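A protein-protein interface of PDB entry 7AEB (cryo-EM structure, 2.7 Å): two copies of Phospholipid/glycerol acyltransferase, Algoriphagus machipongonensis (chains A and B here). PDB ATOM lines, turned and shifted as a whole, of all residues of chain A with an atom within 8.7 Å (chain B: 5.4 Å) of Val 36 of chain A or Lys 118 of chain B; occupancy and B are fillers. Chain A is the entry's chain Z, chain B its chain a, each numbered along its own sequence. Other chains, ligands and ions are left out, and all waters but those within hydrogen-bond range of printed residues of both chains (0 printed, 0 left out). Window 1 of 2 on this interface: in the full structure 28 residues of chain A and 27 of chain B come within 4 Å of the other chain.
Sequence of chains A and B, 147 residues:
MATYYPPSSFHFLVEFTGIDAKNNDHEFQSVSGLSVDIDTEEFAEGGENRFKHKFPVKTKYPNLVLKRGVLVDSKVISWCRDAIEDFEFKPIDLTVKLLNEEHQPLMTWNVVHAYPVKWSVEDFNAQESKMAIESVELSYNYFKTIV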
ATOM      1  N   GLY A  33     -39.600 -20.204  -4.488  1.00  0.00           N
ATOM      2  CA  GLY A  33     -38.777 -20.770  -5.546  1.00  0.00           C
ATOM      3  C   GLY A  33     -37.818 -19.799  -6.224  1.00  0.00           C
ATOM      4  O   GLY A  33     -37.146 -20.175  -7.187  1.00  0.00           O
ATOM      5  N   LEU A  34     -37.699 -18.574  -5.738  1.00  0.00           N
ATOM      6  CA  LEU A  34     -36.801 -17.608  -6.372  1.00  0.00           C
ATOM      7  C   LEU A  34     -35.356 -17.774  -5.894  1.00  0.00           C
ATOM      8  O   LEU A  34     -34.829 -16.954  -5.140  1.00  0.00           O
ATOM      9  CB  LEU A  34     -37.289 -16.192  -6.106  1.00  0.00           C
ATOM     10  CG  LEU A  34     -38.654 -15.798  -6.686  1.00  0.00           C
ATOM     11  CD1 LEU A  34     -39.022 -14.431  -6.194  1.00  0.00           C
ATOM     12  CD2 LEU A  34     -38.628 -15.817  -8.217  1.00  0.00           C
ATOM     13  N   SER A  35     -34.692 -18.834  -6.386  1.00  0.00           N
ATOM     14  CA  SER A  35     -33.305 -19.066  -5.986  1.00  0.00           C
ATOM     15  C   SER A  35     -32.552 -19.735  -7.151  1.00  0.00           C
ATOM     16  O   SER A  35     -33.146 -20.080  -8.174  1.00  0.00           O
ATOM     17  CB  SER A  35     -33.170 -19.992  -4.785  1.00  0.00           C
ATOM     18  OG  SER A  35     -33.744 -21.248  -5.009  1.00  0.00           O
ATOM     19  N   VAL A  36     -31.240 -19.970  -6.963  1.00  0.00           N
ATOM     20  CA  VAL A  36     -30.383 -20.620  -7.974  1.00  0.00           C
ATOM     21  C   VAL A  36     -29.149 -21.300  -7.389  1.00  0.00           C
ATOM     22  O   VAL A  36     -28.726 -20.932  -6.303  1.00  0.00           O
ATOM     23  CB  VAL A  36     -29.906 -19.607  -9.033  1.00  0.00           C
ATOM     24  CG1 VAL A  36     -29.189 -18.440  -8.376  1.00  0.00           C
ATOM     25  CG2 VAL A  36     -29.013 -20.254 -10.061  1.00  0.00           C
ATOM     26  N   ASP A  37     -28.561 -22.301  -8.095  1.00  0.00           N
ATOM     27  CA  ASP A  37     -27.363 -23.017  -7.687  1.00  0.00           C
ATOM     28  C   ASP A  37     -26.463 -23.454  -8.857  1.00  0.00           C
ATOM     29  O   ASP A  37     -26.902 -23.531 -10.002  1.00  0.00           O
ATOM     30  CB  ASP A  37     -27.742 -24.245  -6.857  1.00  0.00           C
ATOM     31  CG  ASP A  37     -28.524 -23.903  -5.601  1.00  0.00           C
ATOM     32  OD1 ASP A  37     -28.955 -24.793  -4.881  1.00  0.00           O
ATOM     33  OD2 ASP A  37     -28.803 -22.835  -5.259  1.00  0.00           O
ATOM     34  N   ILE A  38     -25.200 -23.783  -8.573  1.00  0.00           N
ATOM     35  CA  ILE A  38     -24.298 -24.230  -9.635  1.00  0.00           C
ATOM     36  C   ILE A  38     -23.795 -25.646  -9.384  1.00  0.00           C
ATOM     37  O   ILE A  38     -23.149 -25.910  -8.365  1.00  0.00           O
ATOM     38  CB  ILE A  38     -23.112 -23.276  -9.813  1.00  0.00           C
ATOM     39  CG1 ILE A  38     -23.602 -21.856 -10.085  1.00  0.00           C
ATOM     40  CG2 ILE A  38     -22.217 -23.760 -10.943  1.00  0.00           C
ATOM     41  CD1 ILE A  38     -22.492 -20.849 -10.262  1.00  0.00           C
ATOM     42  N   ASP A  39     -24.068 -26.545 -10.330  1.00  0.00           N
ATOM     43  CA  ASP A  39     -23.542 -27.902 -10.269  1.00  0.00           C
ATOM     44  C   ASP A  39     -22.052 -27.876 -10.499  1.00  0.00           C
ATOM     45  O   ASP A  39     -21.584 -27.215 -11.429  1.00  0.00           O
ATOM     46  CB  ASP A  39     -24.117 -28.817 -11.352  1.00  0.00           C
ATOM     47  CG  ASP A  39     -25.538 -29.241 -11.128  1.00  0.00           C
ATOM     48  OD1 ASP A  39     -26.083 -29.106 -10.040  1.00  0.00           O
ATOM     49  OD2 ASP A  39     -26.108 -29.798 -12.074  1.00  0.00           O
ATOM     50  N   THR A  40     -21.321 -28.684  -9.724  1.00  0.00           N
ATOM     51  CA  THR A  40     -19.877 -28.812  -9.831  1.00  0.00           C
ATOM     52  C   THR A  40     -19.403 -30.264  -9.930  1.00  0.00           C
ATOM     53  O   THR A  40     -20.124 -31.196  -9.596  1.00  0.00           O
ATOM     54  CB  THR A  40     -19.152 -28.179  -8.635  1.00  0.00           C
ATOM     55  OG1 THR A  40     -19.471 -28.916  -7.459  1.00  0.00           O
ATOM     56  CG2 THR A  40     -19.534 -26.723  -8.448  1.00  0.00           C
ATOM     57  N   LYS A  58     -22.974 -26.372 -14.535  1.00  0.00           N
ATOM     58  CA  LYS A  58     -24.262 -25.798 -14.961  1.00  0.00           C
ATOM     59  C   LYS A  58     -24.973 -24.972 -13.892  1.00  0.00           C
ATOM     60  O   LYS A  58     -24.924 -25.281 -12.702  1.00  0.00           O
ATOM     61  CB  LYS A  58     -25.300 -26.853 -15.373  1.00  0.00           C
ATOM     62  CG  LYS A  58     -25.076 -27.609 -16.646  1.00  0.00           C
ATOM     63  CD  LYS A  58     -25.373 -26.784 -17.872  1.00  0.00           C
ATOM     64  CE  LYS A  58     -25.229 -27.632 -19.117  1.00  0.00           C
ATOM     65  NZ  LYS A  58     -25.401 -26.841 -20.353  1.00  0.00           N
ATOM     66  N   THR A  59     -25.727 -23.977 -14.348  1.00  0.00           N
ATOM     67  CA  THR A  59     -26.596 -23.205 -13.471  1.00  0.00           C
ATOM     68  C   THR A  59     -27.972 -23.861 -13.410  1.00  0.00           C
ATOM     69  O   THR A  59     -28.528 -24.242 -14.437  1.00  0.00           O
ATOM     70  CB  THR A  59     -26.718 -21.762 -13.965  1.00  0.00           C
ATOM     71  OG1 THR A  59     -25.430 -21.150 -13.977  1.00  0.00           O
ATOM     72  CG2 THR A  59     -27.567 -20.977 -13.075  1.00  0.00           C
ATOM     73  N   LYS A  60     -28.527 -23.963 -12.205  1.00  0.00           N
ATOM     74  CA  LYS A  60     -29.765 -24.686 -11.955  1.00  0.00           C
ATOM     75  C   LYS A  60     -30.815 -23.845 -11.225  1.00  0.00           C
ATOM     76  O   LYS A  60     -30.489 -23.146 -10.274  1.00  0.00           O
ATOM     77  CB  LYS A  60     -29.378 -25.885 -11.140  1.00  0.00           C
ATOM     78  CG  LYS A  60     -30.392 -26.955 -11.014  1.00  0.00           C
ATOM     79  CD  LYS A  60     -29.846 -28.023 -10.092  1.00  0.00           C
ATOM     80  CE  LYS A  60     -30.897 -29.063  -9.787  1.00  0.00           C
ATOM     81  NZ  LYS A  60     -30.303 -30.212  -9.068  1.00  0.00           N
ATOM     82  N   TYR A  61     -32.083 -23.919 -11.642  1.00  0.00           N
ATOM     83  CA  TYR A  61     -33.182 -23.205 -10.998  1.00  0.00           C
ATOM     84  C   TYR A  61     -34.301 -24.169 -10.596  1.00  0.00           C
ATOM     85  O   TYR A  61     -34.563 -25.121 -11.325  1.00  0.00           O
ATOM     86  CB  TYR A  61     -33.757 -22.147 -11.948  1.00  0.00           C
ATOM     87  CG  TYR A  61     -32.820 -21.057 -12.385  1.00  0.00           C
ATOM     88  CD1 TYR A  61     -31.977 -21.229 -13.464  1.00  0.00           C
ATOM     89  CD2 TYR A  61     -32.824 -19.845 -11.744  1.00  0.00           C
ATOM     90  CE1 TYR A  61     -31.147 -20.231 -13.858  1.00  0.00           C
ATOM     91  CE2 TYR A  61     -32.005 -18.839 -12.141  1.00  0.00           C
ATOM     92  CZ  TYR A  61     -31.170 -19.036 -13.193  1.00  0.00           C
ATOM     93  OH  TYR A  61     -30.338 -18.024 -13.582  1.00  0.00           O
ATOM     94  N   PRO A  62     -34.935 -23.955  -9.436  1.00  0.00           N
ATOM     95  CA  PRO A  62     -36.122 -24.705  -8.983  1.00  0.00           C
ATOM     96  C   PRO A  62     -37.403 -24.151  -9.591  1.00  0.00           C
ATOM     97  O   PRO A  62     -37.431 -23.013 -10.048  1.00  0.00           O
ATOM     98  CB  PRO A  62     -36.110 -24.427  -7.476  1.00  0.00           C
ATOM     99  CG  PRO A  62     -35.528 -23.070  -7.392  1.00  0.00           C
ATOM    100  CD  PRO A  62     -34.495 -22.979  -8.454  1.00  0.00           C
ATOM    101  N   TYR A 140     -39.600 -22.861 -15.548  1.00  0.00           N
ATOM    102  CA  TYR A 140     -39.130 -21.687 -16.298  1.00  0.00           C
ATOM    103  C   TYR A 140     -37.652 -21.881 -16.620  1.00  0.00           C
ATOM    104  O   TYR A 140     -37.022 -22.800 -16.110  1.00  0.00           O
ATOM    105  CB  TYR A 140     -39.391 -20.373 -15.534  1.00  0.00           C
ATOM    106  CG  TYR A 140     -38.690 -20.323 -14.236  1.00  0.00           C
ATOM    107  CD1 TYR A 140     -37.447 -19.733 -14.120  1.00  0.00           C
ATOM    108  CD2 TYR A 140     -39.263 -20.885 -13.125  1.00  0.00           C
ATOM    109  CE1 TYR A 140     -36.790 -19.737 -12.938  1.00  0.00           C
ATOM    110  CE2 TYR A 140     -38.627 -20.890 -11.958  1.00  0.00           C
ATOM    111  CZ  TYR A 140     -37.393 -20.323 -11.855  1.00  0.00           C
ATOM    112  OH  TYR A 140     -36.766 -20.374 -10.647  1.00  0.00           O
ATOM    113  N   ASN A 141     -37.086 -21.021 -17.474  1.00  0.00           N
ATOM    114  CA  ASN A 141     -35.688 -21.213 -17.869  1.00  0.00           C
ATOM    115  C   ASN A 141     -34.688 -20.526 -16.953  1.00  0.00           C
ATOM    116  O   ASN A 141     -33.672 -21.120 -16.588  1.00  0.00           O
ATOM    117  CB  ASN A 141     -35.452 -20.722 -19.286  1.00  0.00           C
ATOM    118  CG  ASN A 141     -36.023 -21.631 -20.317  1.00  0.00           C
ATOM    119  OD1 ASN A 141     -36.263 -22.809 -20.091  1.00  0.00           O
ATOM    120  ND2 ASN A 141     -36.237 -21.088 -21.475  1.00  0.00           N
ATOM    121  N   TYR A 142     -34.935 -19.266 -16.628  1.00  0.00           N
ATOM    122  CA  TYR A 142     -34.038 -18.493 -15.786  1.00  0.00           C
ATOM    123  C   TYR A 142     -34.771 -17.253 -15.323  1.00  0.00           C
ATOM    124  O   TYR A 142     -35.889 -16.971 -15.754  1.00  0.00           O
ATOM    125  CB  TYR A 142     -32.747 -18.102 -16.502  1.00  0.00           C
ATOM    126  CG  TYR A 142     -32.907 -17.234 -17.704  1.00  0.00           C
ATOM    127  CD1 TYR A 142     -32.885 -15.857 -17.593  1.00  0.00           C
ATOM    128  CD2 TYR A 142     -33.039 -17.792 -18.951  1.00  0.00           C
ATOM    129  CE1 TYR A 142     -33.016 -15.073 -18.675  1.00  0.00           C
ATOM    130  CE2 TYR A 142     -33.160 -17.011 -20.048  1.00  0.00           C
ATOM    131  CZ  TYR A 142     -33.149 -15.650 -19.908  1.00  0.00           C
ATOM    132  OH  TYR A 142     -33.272 -14.845 -21.004  1.00  0.00           O
ATOM    133  N   PHE A 143     -34.110 -16.503 -14.455  1.00  0.00           N
ATOM    134  CA  PHE A 143     -34.616 -15.203 -14.086  1.00  0.00           C
ATOM    135  C   PHE A 143     -33.495 -14.189 -13.980  1.00  0.00           C
ATOM    136  O   PHE A 143     -32.338 -14.531 -13.756  1.00  0.00           O
ATOM    137  CB  PHE A 143     -35.462 -15.224 -12.792  1.00  0.00           C
ATOM    138  CG  PHE A 143     -34.723 -15.554 -11.527  1.00  0.00           C
ATOM    139  CD1 PHE A 143     -34.038 -14.588 -10.824  1.00  0.00           C
ATOM    140  CD2 PHE A 143     -34.805 -16.810 -10.984  1.00  0.00           C
ATOM    141  CE1 PHE A 143     -33.399 -14.891  -9.661  1.00  0.00           C
ATOM    142  CE2 PHE A 143     -34.170 -17.108  -9.803  1.00  0.00           C
ATOM    143  CZ  PHE A 143     -33.466 -16.153  -9.150  1.00  0.00           C
ATOM    144  N   ILE B  84     -22.892 -16.195 -11.806  1.00  0.00           N
ATOM    145  CA  ILE B  84     -24.131 -16.960 -11.971  1.00  0.00           C
ATOM    146  C   ILE B  84     -24.690 -16.850 -13.382  1.00  0.00           C
ATOM    147  O   ILE B  84     -25.127 -17.845 -13.975  1.00  0.00           O
ATOM    148  CB  ILE B  84     -25.187 -16.496 -10.954  1.00  0.00           C
ATOM    149  CG1 ILE B  84     -24.778 -16.914  -9.537  1.00  0.00           C
ATOM    150  CG2 ILE B  84     -26.583 -17.043 -11.319  1.00  0.00           C
ATOM    151  CD1 ILE B  84     -25.566 -16.235  -8.417  1.00  0.00           C
ATOM    152  N   PRO B 116     -18.577 -17.795  -5.773  1.00  0.00           N
ATOM    153  CA  PRO B 116     -19.991 -18.094  -5.456  1.00  0.00           C
ATOM    154  C   PRO B 116     -20.566 -19.347  -6.098  1.00  0.00           C
ATOM    155  O   PRO B 116     -20.390 -19.574  -7.287  1.00  0.00           O
ATOM    156  CB  PRO B 116     -20.727 -16.864  -5.984  1.00  0.00           C
ATOM    157  CG  PRO B 116     -19.749 -16.092  -6.790  1.00  0.00           C
ATOM    158  CD  PRO B 116     -18.500 -16.823  -6.876  1.00  0.00           C
ATOM    159  N   VAL B 117     -21.269 -20.157  -5.309  1.00  0.00           N
ATOM    160  CA  VAL B 117     -21.974 -21.318  -5.840  1.00  0.00           C
ATOM    161  C   VAL B 117     -23.466 -21.262  -5.585  1.00  0.00           C
ATOM    162  O   VAL B 117     -24.204 -22.033  -6.196  1.00  0.00           O
ATOM    163  CB  VAL B 117     -21.409 -22.677  -5.344  1.00  0.00           C
ATOM    164  CG1 VAL B 117     -20.111 -23.040  -6.034  1.00  0.00           C
ATOM    165  CG2 VAL B 117     -21.306 -22.780  -3.826  1.00  0.00           C
ATOM    166  N   LYS B 118     -23.948 -20.375  -4.728  1.00  0.00           N
ATOM    167  CA  LYS B 118     -25.371 -20.346  -4.441  1.00  0.00           C
ATOM    168  C   LYS B 118     -25.870 -18.974  -3.984  1.00  0.00           C
ATOM    169  O   LYS B 118     -25.148 -18.241  -3.330  1.00  0.00           O
ATOM    170  CB  LYS B 118     -25.657 -21.387  -3.379  1.00  0.00           C
ATOM    171  CG  LYS B 118     -27.096 -21.548  -3.024  1.00  0.00           C
ATOM    172  CD  LYS B 118     -27.296 -22.834  -2.303  1.00  0.00           C
ATOM    173  CE  LYS B 118     -28.716 -22.931  -1.815  1.00  0.00           C
ATOM    174  NZ  LYS B 118     -29.004 -24.292  -1.310  1.00  0.00           N
ATOM    175  N   TRP B 119     -27.115 -18.636  -4.318  1.00  0.00           N
ATOM    176  CA  TRP B 119     -27.752 -17.401  -3.871  1.00  0.00           C
ATOM    177  C   TRP B 119     -29.255 -17.594  -3.778  1.00  0.00           C
ATOM    178  O   TRP B 119     -29.874 -18.039  -4.747  1.00  0.00           O
ATOM    179  CB  TRP B 119     -27.454 -16.256  -4.832  1.00  0.00           C
ATOM    180  CG  TRP B 119     -28.145 -14.963  -4.497  1.00  0.00           C
ATOM    181  CD1 TRP B 119     -28.316 -14.396  -3.267  1.00  0.00           C
ATOM    182  CD2 TRP B 119     -28.756 -14.079  -5.422  1.00  0.00           C
ATOM    183  NE1 TRP B 119     -28.993 -13.220  -3.378  1.00  0.00           N
ATOM    184  CE2 TRP B 119     -29.279 -13.006  -4.696  1.00  0.00           C
ATOM    185  CE3 TRP B 119     -28.912 -14.092  -6.805  1.00  0.00           C
ATOM    186  CZ2 TRP B 119     -29.941 -11.965  -5.297  1.00  0.00           C
ATOM    187  CZ3 TRP B 119     -29.573 -13.051  -7.405  1.00  0.00           C
ATOM    188  CH2 TRP B 119     -30.078 -12.003  -6.656  1.00  0.00           C
ATOM    189  N   SER B 120     -29.848 -17.230  -2.641  1.00  0.00           N
ATOM    190  CA  SER B 120     -31.294 -17.373  -2.500  1.00  0.00           C
ATOM    191  C   SER B 120     -31.921 -16.380  -1.526  1.00  0.00           C
ATOM    192  O   SER B 120     -31.247 -15.745  -0.710  1.00  0.00           O
ATOM    193  CB  SER B 120     -31.654 -18.780  -2.059  1.00  0.00           C
ATOM    194  OG  SER B 120     -31.173 -19.042  -0.765  1.00  0.00           O
ATOM    195  N   SER B 135     -29.434 -15.243   1.528  1.00  0.00           N
ATOM    196  CA  SER B 135     -28.394 -16.221   1.826  1.00  0.00           C
ATOM    197  C   SER B 135     -27.431 -16.482   0.668  1.00  0.00           C
ATOM    198  O   SER B 135     -27.843 -16.694  -0.476  1.00  0.00           O
ATOM    199  CB  SER B 135     -29.038 -17.526   2.261  1.00  0.00           C
ATOM    200  OG  SER B 135     -28.057 -18.513   2.416  1.00  0.00           O
ATOM    201  N   VAL B 136     -26.128 -16.452   0.980  1.00  0.00           N
ATOM    202  CA  VAL B 136     -25.045 -16.631   0.006  1.00  0.00           C
ATOM    203  C   VAL B 136     -24.059 -17.720   0.439  1.00  0.00           C
ATOM    204  O   VAL B 136     -23.546 -17.706   1.561  1.00  0.00           O
ATOM    205  CB  VAL B 136     -24.296 -15.306  -0.236  1.00  0.00           C
ATOM    206  CG1 VAL B 136     -23.120 -15.499  -1.180  1.00  0.00           C
ATOM    207  CG2 VAL B 136     -25.243 -14.298  -0.831  1.00  0.00           C
ATOM    208  N   GLU B 137     -23.747 -18.634  -0.475  1.00  0.00           N
ATOM    209  CA  GLU B 137     -22.813 -19.712  -0.199  1.00  0.00           C
ATOM    210  C   GLU B 137     -21.612 -19.686  -1.143  1.00  0.00           C
ATOM    211  O   GLU B 137     -21.776 -19.565  -2.363  1.00  0.00           O
ATOM    212  CB  GLU B 137     -23.561 -21.029  -0.262  1.00  0.00           C
ATOM    213  CG  GLU B 137     -22.775 -22.247   0.009  1.00  0.00           C
ATOM    214  CD  GLU B 137     -23.686 -23.424   0.150  1.00  0.00           C
ATOM    215  OE1 GLU B 137     -24.885 -23.200   0.305  1.00  0.00           O
ATOM    216  OE2 GLU B 137     -23.229 -24.567   0.050  1.00  0.00           O
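Among the printed residues, pairs that only touch across the chains: Ser 35 of chain A with Ser 120 of chain B, Asp 37 of chain A with Val 117 of chain B, Val 36 of chain A with Lys 118 of chain B, Ser 35 of chain A with Trp 119 of chain B and Ile 38 of chain A with Pro 116 of chain B.
The backbone NH (N) of Val 36 of chain A lies within hydrogen-bond range of the backbone carbonyl oxygen (O) of Trp 119 of chain B.
The side-chain carboxylate of Asp 37 of chain A lies within salt-bridge range of the side-chain amino group of Lys 118 of chain B (3.6 Å).
The backbone NH of Ile 38 of chain A lies within hydrogen-bond range of the backbone carbonyl oxygen of Val 117 of chain B.
OG1 of Thr 59 of chain A sits at hydrogen-bond distance from O of Ile 84 of chain B (3.3 Å).
The backbone NH of Lys 60 of chain A is in hydrogen-bond range of the backbone carbonyl oxygen of Asp 37 of chain A (2.8 Å).
N of Val 117 of chain B sits at hydrogen-bond distance from O of Glu 137 of chain B (3.0 Å).
O of Lys 118 of chain B sits at hydrogen-bond distance from N of Glu 137 of chain B (3.2 Å).
N of Ser 135 of chain B lies within hydrogen-bond range of O of Ser 120 of chain B (2.9 Å).
No position is printed for both chains.
Of the 9 pairs that touch across the chains among the printed residues, none has its exchanged pair printed and touching as well.
Printed residues of chain B that touch a printed residue of chain A: Ile 84, Pro 116, Val 117, Lys 118, Trp 119 and Ser 120.
Of the 17 printed residues of chain A, 5 touch a printed residue of chain B.
Among the printed residues, 9 pairs touch across the chains.
Among the printed residues, Asp or Glu carboxylates within 4 Å of a Lys or Arg side-chain nitrogen of the other chain: Asp 37 of chain A with Lys 118 of chain B (3.6 Å).
Val 36 of chain A touches just these residues of chain B: Lys 118 and Trp 119.
Asp 39 of chain A touches none of the printed residues of chain B.
Tyr 142 of chain A touches none of the printed residues of chain B.
Of the printed residues of chain A, Val 117 of chain B touches Asp 37 and Ile 38.
Printed residues of chain A within 4 Å of Lys 118 of chain B: Val 36 and Asp 37.
Of the printed residues of chain A, Ser 120 of chain B touches Ser 35 (3.3 Å).
The nearest residue of chain B that does not touch Val 36 of chain A is Ile 84 of chain B (4.2 Å).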
